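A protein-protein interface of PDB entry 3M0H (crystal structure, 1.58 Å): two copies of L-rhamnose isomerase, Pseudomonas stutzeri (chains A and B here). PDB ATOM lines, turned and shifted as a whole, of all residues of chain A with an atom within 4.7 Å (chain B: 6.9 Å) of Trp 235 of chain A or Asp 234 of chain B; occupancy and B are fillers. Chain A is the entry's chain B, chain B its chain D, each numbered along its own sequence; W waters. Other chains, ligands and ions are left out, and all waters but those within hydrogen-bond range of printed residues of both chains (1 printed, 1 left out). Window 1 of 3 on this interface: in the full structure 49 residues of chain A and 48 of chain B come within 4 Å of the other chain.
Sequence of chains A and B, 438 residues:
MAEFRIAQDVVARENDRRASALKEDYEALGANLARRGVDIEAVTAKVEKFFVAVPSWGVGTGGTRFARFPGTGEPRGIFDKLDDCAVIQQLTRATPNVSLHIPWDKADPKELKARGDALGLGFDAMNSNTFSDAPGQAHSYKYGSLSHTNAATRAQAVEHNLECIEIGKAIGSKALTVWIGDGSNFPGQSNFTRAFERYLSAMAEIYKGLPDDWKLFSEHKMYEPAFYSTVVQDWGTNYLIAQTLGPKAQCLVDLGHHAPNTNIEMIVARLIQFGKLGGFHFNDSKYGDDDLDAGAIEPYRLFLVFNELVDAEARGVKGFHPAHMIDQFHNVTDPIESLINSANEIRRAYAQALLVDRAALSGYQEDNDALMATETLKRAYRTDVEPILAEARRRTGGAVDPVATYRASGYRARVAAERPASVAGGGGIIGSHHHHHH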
ATOM      1  N   HIS A 220     -18.524  -4.254   9.992  1.00  0.00           N
ATOM      2  CA  HIS A 220     -18.358  -5.440  10.827  1.00  0.00           C
ATOM      3  C   HIS A 220     -19.585  -6.342  10.774  1.00  0.00           C
ATOM      4  O   HIS A 220     -20.684  -5.901  10.445  1.00  0.00           O
ATOM      5  CB  HIS A 220     -18.069  -5.055  12.287  1.00  0.00           C
ATOM      6  CG  HIS A 220     -19.142  -4.226  12.924  1.00  0.00           C
ATOM      7  ND1 HIS A 220     -19.128  -2.848  12.905  1.00  0.00           N
ATOM      8  CD2 HIS A 220     -20.263  -4.583  13.594  1.00  0.00           C
ATOM      9  CE1 HIS A 220     -20.194  -2.391  13.539  1.00  0.00           C
ATOM     10  NE2 HIS A 220     -20.899  -3.424  13.966  1.00  0.00           N
ATOM     11  N   ASP A 234     -16.842  -7.336  15.016  1.00  0.00           N
ATOM     12  CA  ASP A 234     -17.656  -6.381  15.762  1.00  0.00           C
ATOM     13  C   ASP A 234     -17.127  -4.958  15.678  1.00  0.00           C
ATOM     14  O   ASP A 234     -16.124  -4.702  15.011  1.00  0.00           O
ATOM     15  CB  ASP A 234     -17.824  -6.806  17.233  1.00  0.00           C
ATOM     16  CG  ASP A 234     -16.515  -6.871  17.999  1.00  0.00           C
ATOM     17  OD1 ASP A 234     -15.529  -6.209  17.616  1.00  0.00           O
ATOM     18  OD2 ASP A 234     -16.490  -7.584  19.024  1.00  0.00           O
ATOM     19  N   TRP A 235     -17.806  -4.034  16.358  1.00  0.00           N
ATOM     20  CA  TRP A 235     -17.408  -2.635  16.309  1.00  0.00           C
ATOM     21  C   TRP A 235     -16.064  -2.349  16.965  1.00  0.00           C
ATOM     22  O   TRP A 235     -15.430  -1.346  16.652  1.00  0.00           O
ATOM     23  CB  TRP A 235     -18.495  -1.740  16.919  1.00  0.00           C
ATOM     24  CG  TRP A 235     -18.456  -1.625  18.410  1.00  0.00           C
ATOM     25  CD1 TRP A 235     -18.955  -2.511  19.320  1.00  0.00           C
ATOM     26  CD2 TRP A 235     -17.886  -0.550  19.165  1.00  0.00           C
ATOM     27  NE1 TRP A 235     -18.733  -2.053  20.598  1.00  0.00           N
ATOM     28  CE2 TRP A 235     -18.078  -0.851  20.531  1.00  0.00           C
ATOM     29  CE3 TRP A 235     -17.231   0.638  18.819  1.00  0.00           C
ATOM     30  CZ2 TRP A 235     -17.639  -0.003  21.556  1.00  0.00           C
ATOM     31  CZ3 TRP A 235     -16.793   1.482  19.836  1.00  0.00           C
ATOM     32  CH2 TRP A 235     -17.001   1.155  21.189  1.00  0.00           C
ATOM     33  N   GLY A 236     -15.635  -3.227  17.867  1.00  0.00           N
ATOM     34  CA  GLY A 236     -14.350  -3.044  18.520  1.00  0.00           C
ATOM     35  C   GLY A 236     -13.248  -3.217  17.492  1.00  0.00           C
ATOM     36  O   GLY A 236     -12.347  -2.386  17.372  1.00  0.00           O
ATOM     37  N   THR A 237     -13.317  -4.309  16.739  1.00  0.00           N
ATOM     38  CA  THR A 237     -12.327  -4.556  15.703  1.00  0.00           C
ATOM     39  C   THR A 237     -12.467  -3.465  14.650  1.00  0.00           C
ATOM     40  O   THR A 237     -11.477  -2.971  14.118  1.00  0.00           O
ATOM     41  CB  THR A 237     -12.536  -5.937  15.053  1.00  0.00           C
ATOM     42  OG1 THR A 237     -12.199  -6.955  16.001  1.00  0.00           O
ATOM     43  CG2 THR A 237     -11.666  -6.095  13.813  1.00  0.00           C
ATOM     44  N   ASN A 238     -13.706  -3.076  14.366  1.00  0.00           N
ATOM     45  CA  ASN A 238     -13.949  -2.042  13.370  1.00  0.00           C
ATOM     46  C   ASN A 238     -13.282  -0.732  13.789  1.00  0.00           C
ATOM     47  O   ASN A 238     -12.690  -0.035  12.960  1.00  0.00           O
ATOM     48  CB  ASN A 238     -15.455  -1.834  13.169  1.00  0.00           C
ATOM     49  CG  ASN A 238     -15.796  -1.426  11.749  1.00  0.00           C
ATOM     50  OD1 ASN A 238     -14.907  -1.134  10.951  1.00  0.00           O
ATOM     51  ND2 ASN A 238     -17.083  -1.403  11.427  1.00  0.00           N
ATOM     52  N   TYR A 239     -13.362  -0.398  15.073  1.00  0.00           N
ATOM     53  CA  TYR A 239     -12.732   0.829  15.547  1.00  0.00           C
ATOM     54  C   TYR A 239     -11.219   0.745  15.359  1.00  0.00           C
ATOM     55  O   TYR A 239     -10.586   1.708  14.927  1.00  0.00           O
ATOM     56  CB  TYR A 239     -13.033   1.084  17.023  1.00  0.00           C
ATOM     57  CG  TYR A 239     -12.359   2.347  17.511  1.00  0.00           C
ATOM     58  CD1 TYR A 239     -12.862   3.600  17.169  1.00  0.00           C
ATOM     59  CD2 TYR A 239     -11.172   2.288  18.241  1.00  0.00           C
ATOM     60  CE1 TYR A 239     -12.200   4.766  17.534  1.00  0.00           C
ATOM     61  CE2 TYR A 239     -10.499   3.450  18.612  1.00  0.00           C
ATOM     62  CZ  TYR A 239     -11.020   4.682  18.254  1.00  0.00           C
ATOM     63  OH  TYR A 239     -10.361   5.836  18.612  1.00  0.00           O
ATOM     64  N   ILE A 267     -23.399   1.594  20.689  1.00  0.00           N
ATOM     65  CA  ILE A 267     -22.279   1.469  19.762  1.00  0.00           C
ATOM     66  C   ILE A 267     -22.246   2.716  18.881  1.00  0.00           C
ATOM     67  O   ILE A 267     -21.185   3.290  18.626  1.00  0.00           O
ATOM     68  CB  ILE A 267     -22.427   0.211  18.879  1.00  0.00           C
ATOM     69  CG1 ILE A 267     -22.230  -1.038  19.740  1.00  0.00           C
ATOM     70  CG2 ILE A 267     -21.429   0.255  17.723  1.00  0.00           C
ATOM     71  CD1 ILE A 267     -22.478  -2.340  19.006  1.00  0.00           C
ATOM     72  N   ARG A 270     -20.843   5.646  20.855  1.00  0.00           N
ATOM     73  CA  ARG A 270     -19.398   5.519  21.035  1.00  0.00           C
ATOM     74  C   ARG A 270     -18.637   5.914  19.772  1.00  0.00           C
ATOM     75  O   ARG A 270     -17.654   6.660  19.828  1.00  0.00           O
ATOM     76  CB  ARG A 270     -19.040   4.082  21.430  1.00  0.00           C
ATOM     77  CG  ARG A 270     -19.542   3.649  22.812  1.00  0.00           C
ATOM     78  CD  ARG A 270     -18.685   4.220  23.949  1.00  0.00           C
ATOM     79  NE  ARG A 270     -19.107   3.731  25.265  1.00  0.00           N
ATOM     80  CZ  ARG A 270     -20.021   4.316  26.036  1.00  0.00           C
ATOM     81  NH1 ARG A 270     -20.629   5.430  25.637  1.00  0.00           N
ATOM     82  NH2 ARG A 270     -20.333   3.784  27.210  1.00  0.00           N
ATOM     83  N   LEU A 271     -19.087   5.416  18.626  1.00  0.00           N
ATOM     84  CA  LEU A 271     -18.424   5.747  17.370  1.00  0.00           C
ATOM     85  C   LEU A 271     -18.523   7.244  17.067  1.00  0.00           C
ATOM     86  O   LEU A 271     -17.583   7.837  16.540  1.00  0.00           O
ATOM     87  CB  LEU A 271     -19.019   4.919  16.228  1.00  0.00           C
ATOM     88  CG  LEU A 271     -18.644   3.431  16.244  1.00  0.00           C
ATOM     89  CD1 LEU A 271     -19.488   2.682  15.223  1.00  0.00           C
ATOM     90  CD2 LEU A 271     -17.151   3.262  15.951  1.00  0.00           C
ATOM     91  N   GLU B 219     -12.893  -3.638  33.939  1.00  0.00           N
ATOM     92  CA  GLU B 219     -13.619  -4.845  33.561  1.00  0.00           C
ATOM     93  C   GLU B 219     -14.975  -4.551  32.925  1.00  0.00           C
ATOM     94  O   GLU B 219     -15.867  -4.005  33.572  1.00  0.00           O
ATOM     95  CB  GLU B 219     -13.787  -5.713  34.811  1.00  0.00           C
ATOM     96  CG  GLU B 219     -14.647  -6.940  34.632  1.00  0.00           C
ATOM     97  CD  GLU B 219     -14.721  -7.770  35.895  1.00  0.00           C
ATOM     98  OE1 GLU B 219     -14.338  -7.254  36.971  1.00  0.00           O
ATOM     99  OE2 GLU B 219     -15.171  -8.931  35.815  1.00  0.00           O
ATOM    100  N   HIS B 220     -15.127  -4.904  31.651  1.00  0.00           N
ATOM    101  CA  HIS B 220     -16.387  -4.668  30.955  1.00  0.00           C
ATOM    102  C   HIS B 220     -17.423  -5.737  31.285  1.00  0.00           C
ATOM    103  O   HIS B 220     -17.082  -6.843  31.708  1.00  0.00           O
ATOM    104  CB  HIS B 220     -16.169  -4.605  29.432  1.00  0.00           C
ATOM    105  CG  HIS B 220     -15.589  -5.857  28.840  1.00  0.00           C
ATOM    106  ND1 HIS B 220     -14.233  -6.046  28.671  1.00  0.00           N
ATOM    107  CD2 HIS B 220     -16.184  -6.981  28.374  1.00  0.00           C
ATOM    108  CE1 HIS B 220     -14.018  -7.231  28.128  1.00  0.00           C
ATOM    109  NE2 HIS B 220     -15.185  -7.820  27.936  1.00  0.00           N
ATOM    110  N   LYS B 221     -18.692  -5.392  31.101  1.00  0.00           N
ATOM    111  CA  LYS B 221     -19.789  -6.318  31.359  1.00  0.00           C
ATOM    112  C   LYS B 221     -20.996  -5.835  30.567  1.00  0.00           C
ATOM    113  O   LYS B 221     -21.373  -4.666  30.649  1.00  0.00           O
ATOM    114  CB  LYS B 221     -20.114  -6.362  32.856  1.00  0.00           C
ATOM    115  CG  LYS B 221     -21.073  -7.482  33.223  1.00  0.00           C
ATOM    116  CD  LYS B 221     -21.299  -7.576  34.721  1.00  0.00           C
ATOM    117  CE  LYS B 221     -22.212  -8.747  35.044  1.00  0.00           C
ATOM    118  NZ  LYS B 221     -22.562  -8.812  36.486  1.00  0.00           N
ATOM    119  N   MET B 222     -21.604  -6.737  29.803  1.00  0.00           N
ATOM    120  CA  MET B 222     -22.747  -6.377  28.969  1.00  0.00           C
ATOM    121  C   MET B 222     -23.950  -5.848  29.749  1.00  0.00           C
ATOM    122  O   MET B 222     -24.580  -4.869  29.340  1.00  0.00           O
ATOM    123  CB  MET B 222     -23.174  -7.576  28.126  1.00  0.00           C
ATOM    124  CG  MET B 222     -24.321  -7.283  27.184  1.00  0.00           C
ATOM    125  SD  MET B 222     -24.850  -8.778  26.343  1.00  0.00           S
ATOM    126  CE  MET B 222     -25.655  -8.097  24.910  1.00  0.00           C
ATOM    127  N   THR B 230     -24.949  -0.202  29.958  1.00  0.00           N
ATOM    128  CA  THR B 230     -23.872  -0.252  30.937  1.00  0.00           C
ATOM    129  C   THR B 230     -22.755   0.600  30.348  1.00  0.00           C
ATOM    130  O   THR B 230     -22.461   0.505  29.156  1.00  0.00           O
ATOM    131  CB  THR B 230     -23.400  -1.706  31.168  1.00  0.00           C
ATOM    132  OG1 THR B 230     -24.422  -2.430  31.866  1.00  0.00           O
ATOM    133  CG2 THR B 230     -22.121  -1.737  31.994  1.00  0.00           C
ATOM    134  N   VAL B 231     -22.150   1.454  31.169  1.00  0.00           N
ATOM    135  CA  VAL B 231     -21.096   2.330  30.672  1.00  0.00           C
ATOM    136  C   VAL B 231     -19.938   1.534  30.070  1.00  0.00           C
ATOM    137  O   VAL B 231     -19.551   1.761  28.925  1.00  0.00           O
ATOM    138  CB  VAL B 231     -20.584   3.271  31.783  1.00  0.00           C
ATOM    139  CG1 VAL B 231     -19.496   4.183  31.236  1.00  0.00           C
ATOM    140  CG2 VAL B 231     -21.737   4.119  32.309  1.00  0.00           C
ATOM    141  N   VAL B 232     -19.385   0.601  30.834  1.00  0.00           N
ATOM    142  CA  VAL B 232     -18.294  -0.225  30.327  1.00  0.00           C
ATOM    143  C   VAL B 232     -18.966  -1.539  29.941  1.00  0.00           C
ATOM    144  O   VAL B 232     -18.856  -2.543  30.650  1.00  0.00           O
ATOM    145  CB  VAL B 232     -17.223  -0.461  31.414  1.00  0.00           C
ATOM    146  CG1 VAL B 232     -16.000  -1.119  30.798  1.00  0.00           C
ATOM    147  CG2 VAL B 232     -16.843   0.863  32.069  1.00  0.00           C
ATOM    148  N   GLN B 233     -19.655  -1.520  28.801  1.00  0.00           N
ATOM    149  CA  GLN B 233     -20.423  -2.672  28.345  1.00  0.00           C
ATOM    150  C   GLN B 233     -19.707  -3.770  27.565  1.00  0.00           C
ATOM    151  O   GLN B 233     -20.135  -4.923  27.607  1.00  0.00           O
ATOM    152  CB  GLN B 233     -21.651  -2.194  27.554  1.00  0.00           C
ATOM    153  CG  GLN B 233     -21.518  -2.268  26.039  1.00  0.00           C
ATOM    154  CD  GLN B 233     -20.628  -1.189  25.445  1.00  0.00           C
ATOM    155  OE1 GLN B 233     -19.699  -0.701  26.089  1.00  0.00           O
ATOM    156  NE2 GLN B 233     -20.899  -0.829  24.197  1.00  0.00           N
ATOM    157  N   ASP B 234     -18.647  -3.437  26.842  1.00  0.00           N
ATOM    158  CA  ASP B 234     -17.936  -4.474  26.097  1.00  0.00           C
ATOM    159  C   ASP B 234     -16.460  -4.159  25.914  1.00  0.00           C
ATOM    160  O   ASP B 234     -15.970  -3.137  26.400  1.00  0.00           O
ATOM    161  CB  ASP B 234     -18.604  -4.746  24.737  1.00  0.00           C
ATOM    162  CG  ASP B 234     -18.607  -3.541  23.815  1.00  0.00           C
ATOM    163  OD1 ASP B 234     -17.765  -2.640  23.985  1.00  0.00           O
ATOM    164  OD2 ASP B 234     -19.451  -3.508  22.893  1.00  0.00           O
ATOM    165  N   TRP B 235     -15.747  -5.041  25.220  1.00  0.00           N
ATOM    166  CA  TRP B 235     -14.315  -4.857  25.036  1.00  0.00           C
ATOM    167  C   TRP B 235     -13.934  -3.656  24.176  1.00  0.00           C
ATOM    168  O   TRP B 235     -12.816  -3.149  24.281  1.00  0.00           O
ATOM    169  CB  TRP B 235     -13.676  -6.134  24.475  1.00  0.00           C
ATOM    170  CG  TRP B 235     -13.818  -6.327  22.997  1.00  0.00           C
ATOM    171  CD1 TRP B 235     -14.899  -6.822  22.326  1.00  0.00           C
ATOM    172  CD2 TRP B 235     -12.828  -6.033  22.006  1.00  0.00           C
ATOM    173  NE1 TRP B 235     -14.641  -6.857  20.973  1.00  0.00           N
ATOM    174  CE2 TRP B 235     -13.376  -6.379  20.751  1.00  0.00           C
ATOM    175  CE3 TRP B 235     -11.529  -5.512  22.056  1.00  0.00           C
ATOM    176  CZ2 TRP B 235     -12.668  -6.219  19.555  1.00  0.00           C
ATOM    177  CZ3 TRP B 235     -10.825  -5.352  20.863  1.00  0.00           C
ATOM    178  CH2 TRP B 235     -11.397  -5.705  19.632  1.00  0.00           C
ATOM    179  N   GLY B 236     -14.855  -3.205  23.332  1.00  0.00           N
ATOM    180  CA  GLY B 236     -14.581  -2.051  22.494  1.00  0.00           C
ATOM    181  C   GLY B 236     -14.466  -0.818  23.366  1.00  0.00           C
ATOM    182  O   GLY B 236     -13.500  -0.056  23.268  1.00  0.00           O
ATOM    183  N   THR B 237     -15.462  -0.611  24.222  1.00  0.00           N
ATOM    184  CA  THR B 237     -15.440   0.520  25.139  1.00  0.00           C
ATOM    185  C   THR B 237     -14.243   0.352  26.070  1.00  0.00           C
ATOM    186  O   THR B 237     -13.553   1.318  26.392  1.00  0.00           O
ATOM    187  CB  THR B 237     -16.736   0.590  25.982  1.00  0.00           C
ATOM    188  OG1 THR B 237     -17.826   0.984  25.142  1.00  0.00           O
ATOM    189  CG2 THR B 237     -16.593   1.600  27.123  1.00  0.00           C
ATOM    190  N   ASN B 238     -13.983  -0.884  26.485  1.00  0.00           N
ATOM    191  CA  ASN B 238     -12.866  -1.158  27.382  1.00  0.00           C
ATOM    192  C   ASN B 238     -11.544  -0.733  26.731  1.00  0.00           C
ATOM    193  O   ASN B 238     -10.690  -0.126  27.381  1.00  0.00           O
ATOM    194  CB  ASN B 238     -12.844  -2.652  27.744  1.00  0.00           C
ATOM    195  CG  ASN B 238     -12.325  -2.904  29.150  1.00  0.00           C
ATOM    196  OD1 ASN B 238     -12.339  -4.039  29.642  1.00  0.00           O
ATOM    197  ND2 ASN B 238     -11.866  -1.846  29.806  1.00  0.00           N
ATOM    198  N   TYR B 239     -11.378  -1.041  25.446  1.00  0.00           N
ATOM    199  CA  TYR B 239     -10.156  -0.658  24.748  1.00  0.00           C
ATOM    200  C   TYR B 239     -10.015   0.863  24.733  1.00  0.00           C
ATOM    201  O   TYR B 239      -8.929   1.397  24.969  1.00  0.00           O
ATOM    202  CB  TYR B 239     -10.155  -1.168  23.307  1.00  0.00           C
ATOM    203  CG  TYR B 239      -8.939  -0.696  22.551  1.00  0.00           C
ATOM    204  CD1 TYR B 239      -7.686  -1.267  22.778  1.00  0.00           C
ATOM    205  CD2 TYR B 239      -9.024   0.378  21.666  1.00  0.00           C
ATOM    206  CE1 TYR B 239      -6.545  -0.773  22.142  1.00  0.00           C
ATOM    207  CE2 TYR B 239      -7.891   0.878  21.028  1.00  0.00           C
ATOM    208  CZ  TYR B 239      -6.658   0.298  21.272  1.00  0.00           C
ATOM    209  OH  TYR B 239      -5.539   0.797  20.642  1.00  0.00           O
ATOM    210  N   LEU B 240     -11.112   1.557  24.442  1.00  0.00           N
ATOM    211  CA  LEU B 240     -11.092   3.017  24.409  1.00  0.00           C
ATOM    212  C   LEU B 240     -10.656   3.563  25.768  1.00  0.00           C
ATOM    213  O   LEU B 240      -9.919   4.546  25.846  1.00  0.00           O
ATOM    214  CB  LEU B 240     -12.478   3.563  24.041  1.00  0.00           C
ATOM    215  CG  LEU B 240     -12.938   3.281  22.606  1.00  0.00           C
ATOM    216  CD1 LEU B 240     -14.386   3.713  22.422  1.00  0.00           C
ATOM    217  CD2 LEU B 240     -12.035   4.023  21.633  1.00  0.00           C
ATOM    218  N   ILE B 241     -11.109   2.914  26.835  1.00  0.00           N
ATOM    219  CA  ILE B 241     -10.748   3.335  28.186  1.00  0.00           C
ATOM    220  C   ILE B 241      -9.251   3.165  28.423  1.00  0.00           C
ATOM    221  O   ILE B 241      -8.562   4.114  28.788  1.00  0.00           O
ATOM    222  CB  ILE B 241     -11.511   2.514  29.250  1.00  0.00           C
ATOM    223  CG1 ILE B 241     -13.007   2.815  29.150  1.00  0.00           C
ATOM    224  CG2 ILE B 241     -10.974   2.835  30.654  1.00  0.00           C
ATOM    225  CD1 ILE B 241     -13.872   1.852  29.936  1.00  0.00           C
ATOM    226  N   HIS B 257     -19.046 -12.302  30.812  1.00  0.00           N
ATOM    227  CA  HIS B 257     -19.568 -10.951  30.614  1.00  0.00           C
ATOM    228  C   HIS B 257     -19.853 -10.553  29.172  1.00  0.00           C
ATOM    229  O   HIS B 257     -19.927  -9.363  28.860  1.00  0.00           O
ATOM    230  CB  HIS B 257     -18.601  -9.931  31.216  1.00  0.00           C
ATOM    231  CG  HIS B 257     -18.555  -9.953  32.711  1.00  0.00           C
ATOM    232  ND1 HIS B 257     -17.916  -8.978  33.447  1.00  0.00           N
ATOM    233  CD2 HIS B 257     -19.073 -10.825  33.607  1.00  0.00           C
ATOM    234  CE1 HIS B 257     -18.045  -9.249  34.734  1.00  0.00           C
ATOM    235  NE2 HIS B 257     -18.744 -10.363  34.859  1.00  0.00           N
ATOM    236  N   HIS B 258     -20.043 -11.537  28.303  1.00  0.00           N
ATOM    237  CA  HIS B 258     -20.277 -11.250  26.899  1.00  0.00           C
ATOM    238  C   HIS B 258     -21.644 -11.676  26.379  1.00  0.00           C
ATOM    239  O   HIS B 258     -22.310 -12.538  26.961  1.00  0.00           O
ATOM    240  CB  HIS B 258     -19.159 -11.894  26.068  1.00  0.00           C
ATOM    241  CG  HIS B 258     -17.785 -11.522  26.534  1.00  0.00           C
ATOM    242  ND1 HIS B 258     -17.157 -12.160  27.582  1.00  0.00           N
ATOM    243  CD2 HIS B 258     -16.953 -10.526  26.147  1.00  0.00           C
ATOM    244  CE1 HIS B 258     -15.999 -11.570  27.823  1.00  0.00           C
ATOM    245  NE2 HIS B 258     -15.851 -10.575  26.967  1.00  0.00           N
ATOM    246  N   ILE B 267     -11.637 -11.939  21.103  1.00  0.00           N
ATOM    247  CA  ILE B 267     -11.472 -10.697  21.850  1.00  0.00           C
ATOM    248  C   ILE B 267     -10.113 -10.746  22.538  1.00  0.00           C
ATOM    249  O   ILE B 267      -9.375  -9.759  22.568  1.00  0.00           O
ATOM    250  CB  ILE B 267     -12.581 -10.531  22.908  1.00  0.00           C
ATOM    251  CG1 ILE B 267     -13.911 -10.250  22.208  1.00  0.00           C
ATOM    252  CG2 ILE B 267     -12.221  -9.409  23.883  1.00  0.00           C
ATOM    253  CD1 ILE B 267     -15.102 -10.234  23.140  1.00  0.00           C
HETATM  254  O   HOH W   1     -18.508  -6.059  21.023  1.00  0.00           O
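Of chain B, only Asp 234 (2.8 Å), Gly 236 (3.7 Å), Thr 237 (3.5 Å) and Leu 240 (3.9 Å) come within 4 Å of Trp 235 of chain A.
Printed residues of chain B within 4 Å of Tyr 239 of chain A: Leu 240 (3.4 Å).
Of the printed residues of chain A, Val 231 of chain B touches Arg 270 (2.8 Å).
Val 232 of chain B touches none of the printed residues of chain A.
Of chain A, only Trp 235 comes within 4 Å of Asp 234 of chain B.
Of the printed residues of chain A, Gly 236 of chain B touches Trp 235 (3.7 Å).
Of the printed residues of chain A, Leu 240 of chain B touches Trp 235 and Tyr 239.
The nearest residue of chain B that does not touch Trp 235 of chain A is Gln 233 of chain B (4.3 Å).
Among the printed residues, pairs that only touch across the chains: Tyr 239 of chain A with Leu 240 of chain B, Thr 237 of chain A with Trp 235 of chain B, Trp 235 of chain A with Thr 237 of chain B, Gly 236 of chain A with Trp 235 of chain B, Trp 235 of chain A with Gly 236 of chain B and Trp 235 of chain A with Leu 240 of chain B.
The side-chain carboxylate of Asp 234 of chain A is in hydrogen-bond range of the indole nitrogen of Trp 235 of chain B (2.8 Å).
NE1 of Trp 235 of chain A lies within hydrogen-bond range of OD2 of Asp 234 of chain B, at 2.8 Å.
O of Val 231 of chain B is in hydrogen-bond range of NH2 of Arg 270 of chain A (2.8 Å).
NE of Arg 270 of chain A is in hydrogen-bond range of OG1 of Thr 237 of chain B, 3.0 Å away.
Asp 234 of chain A touches Trp 235 of chain B, and with the chains exchanged Trp 235 of chain A touches Asp 234 of chain B.
Trp 235 of chain A touches Gly 236 of chain B, and with the chains exchanged Gly 236 of chain A touches Trp 235 of chain B.
Trp 235 of chain A touches Thr 237 of chain B, and with the chains exchanged Thr 237 of chain A touches Trp 235 of chain B.
8 positions are printed for both chains.
Of the 10 pairs that touch across the chains among the printed residues, 6 have their exchanged pair printed and touching as well.
Water W1 lies within hydrogen-bond range of OD2 of Asp 234 of chain A (3.2 Å) and OD2 of Asp 234 of chain B (3.3 Å).
Of the 10 printed residues of chain A, 6 touch a printed residue of chain B.
Hydrophobic or aromatic side chains of chain A that line the printed part of chain B: Trp 235 and Tyr 239.
The backbone NH of Gly 236 of chain A is in hydrogen-bond range of the side-chain carboxylate of Asp 234 of chain A (3.0 Å).
OD1 of Asp 234 of chain A sits at hydrogen-bond distance from N of Thr 237 of chain A.
NE2 of Gln 233 of chain B sits at hydrogen-bond distance from OD2 of Asp 234 of chain B, at 3.3 Å.
The side-chain amide oxygen of Gln 233 of chain B is in hydrogen-bond range of the side-chain hydroxyl of Thr 237 of chain B, 2.7 Å away.
N of Gly 236 of chain B lies within hydrogen-bond range of OD1 of Asp 234 of chain B.
The side-chain carboxylate of Asp 234 of chain B sits at hydrogen-bond distance from the backbone NH of Thr 237 of chain B.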
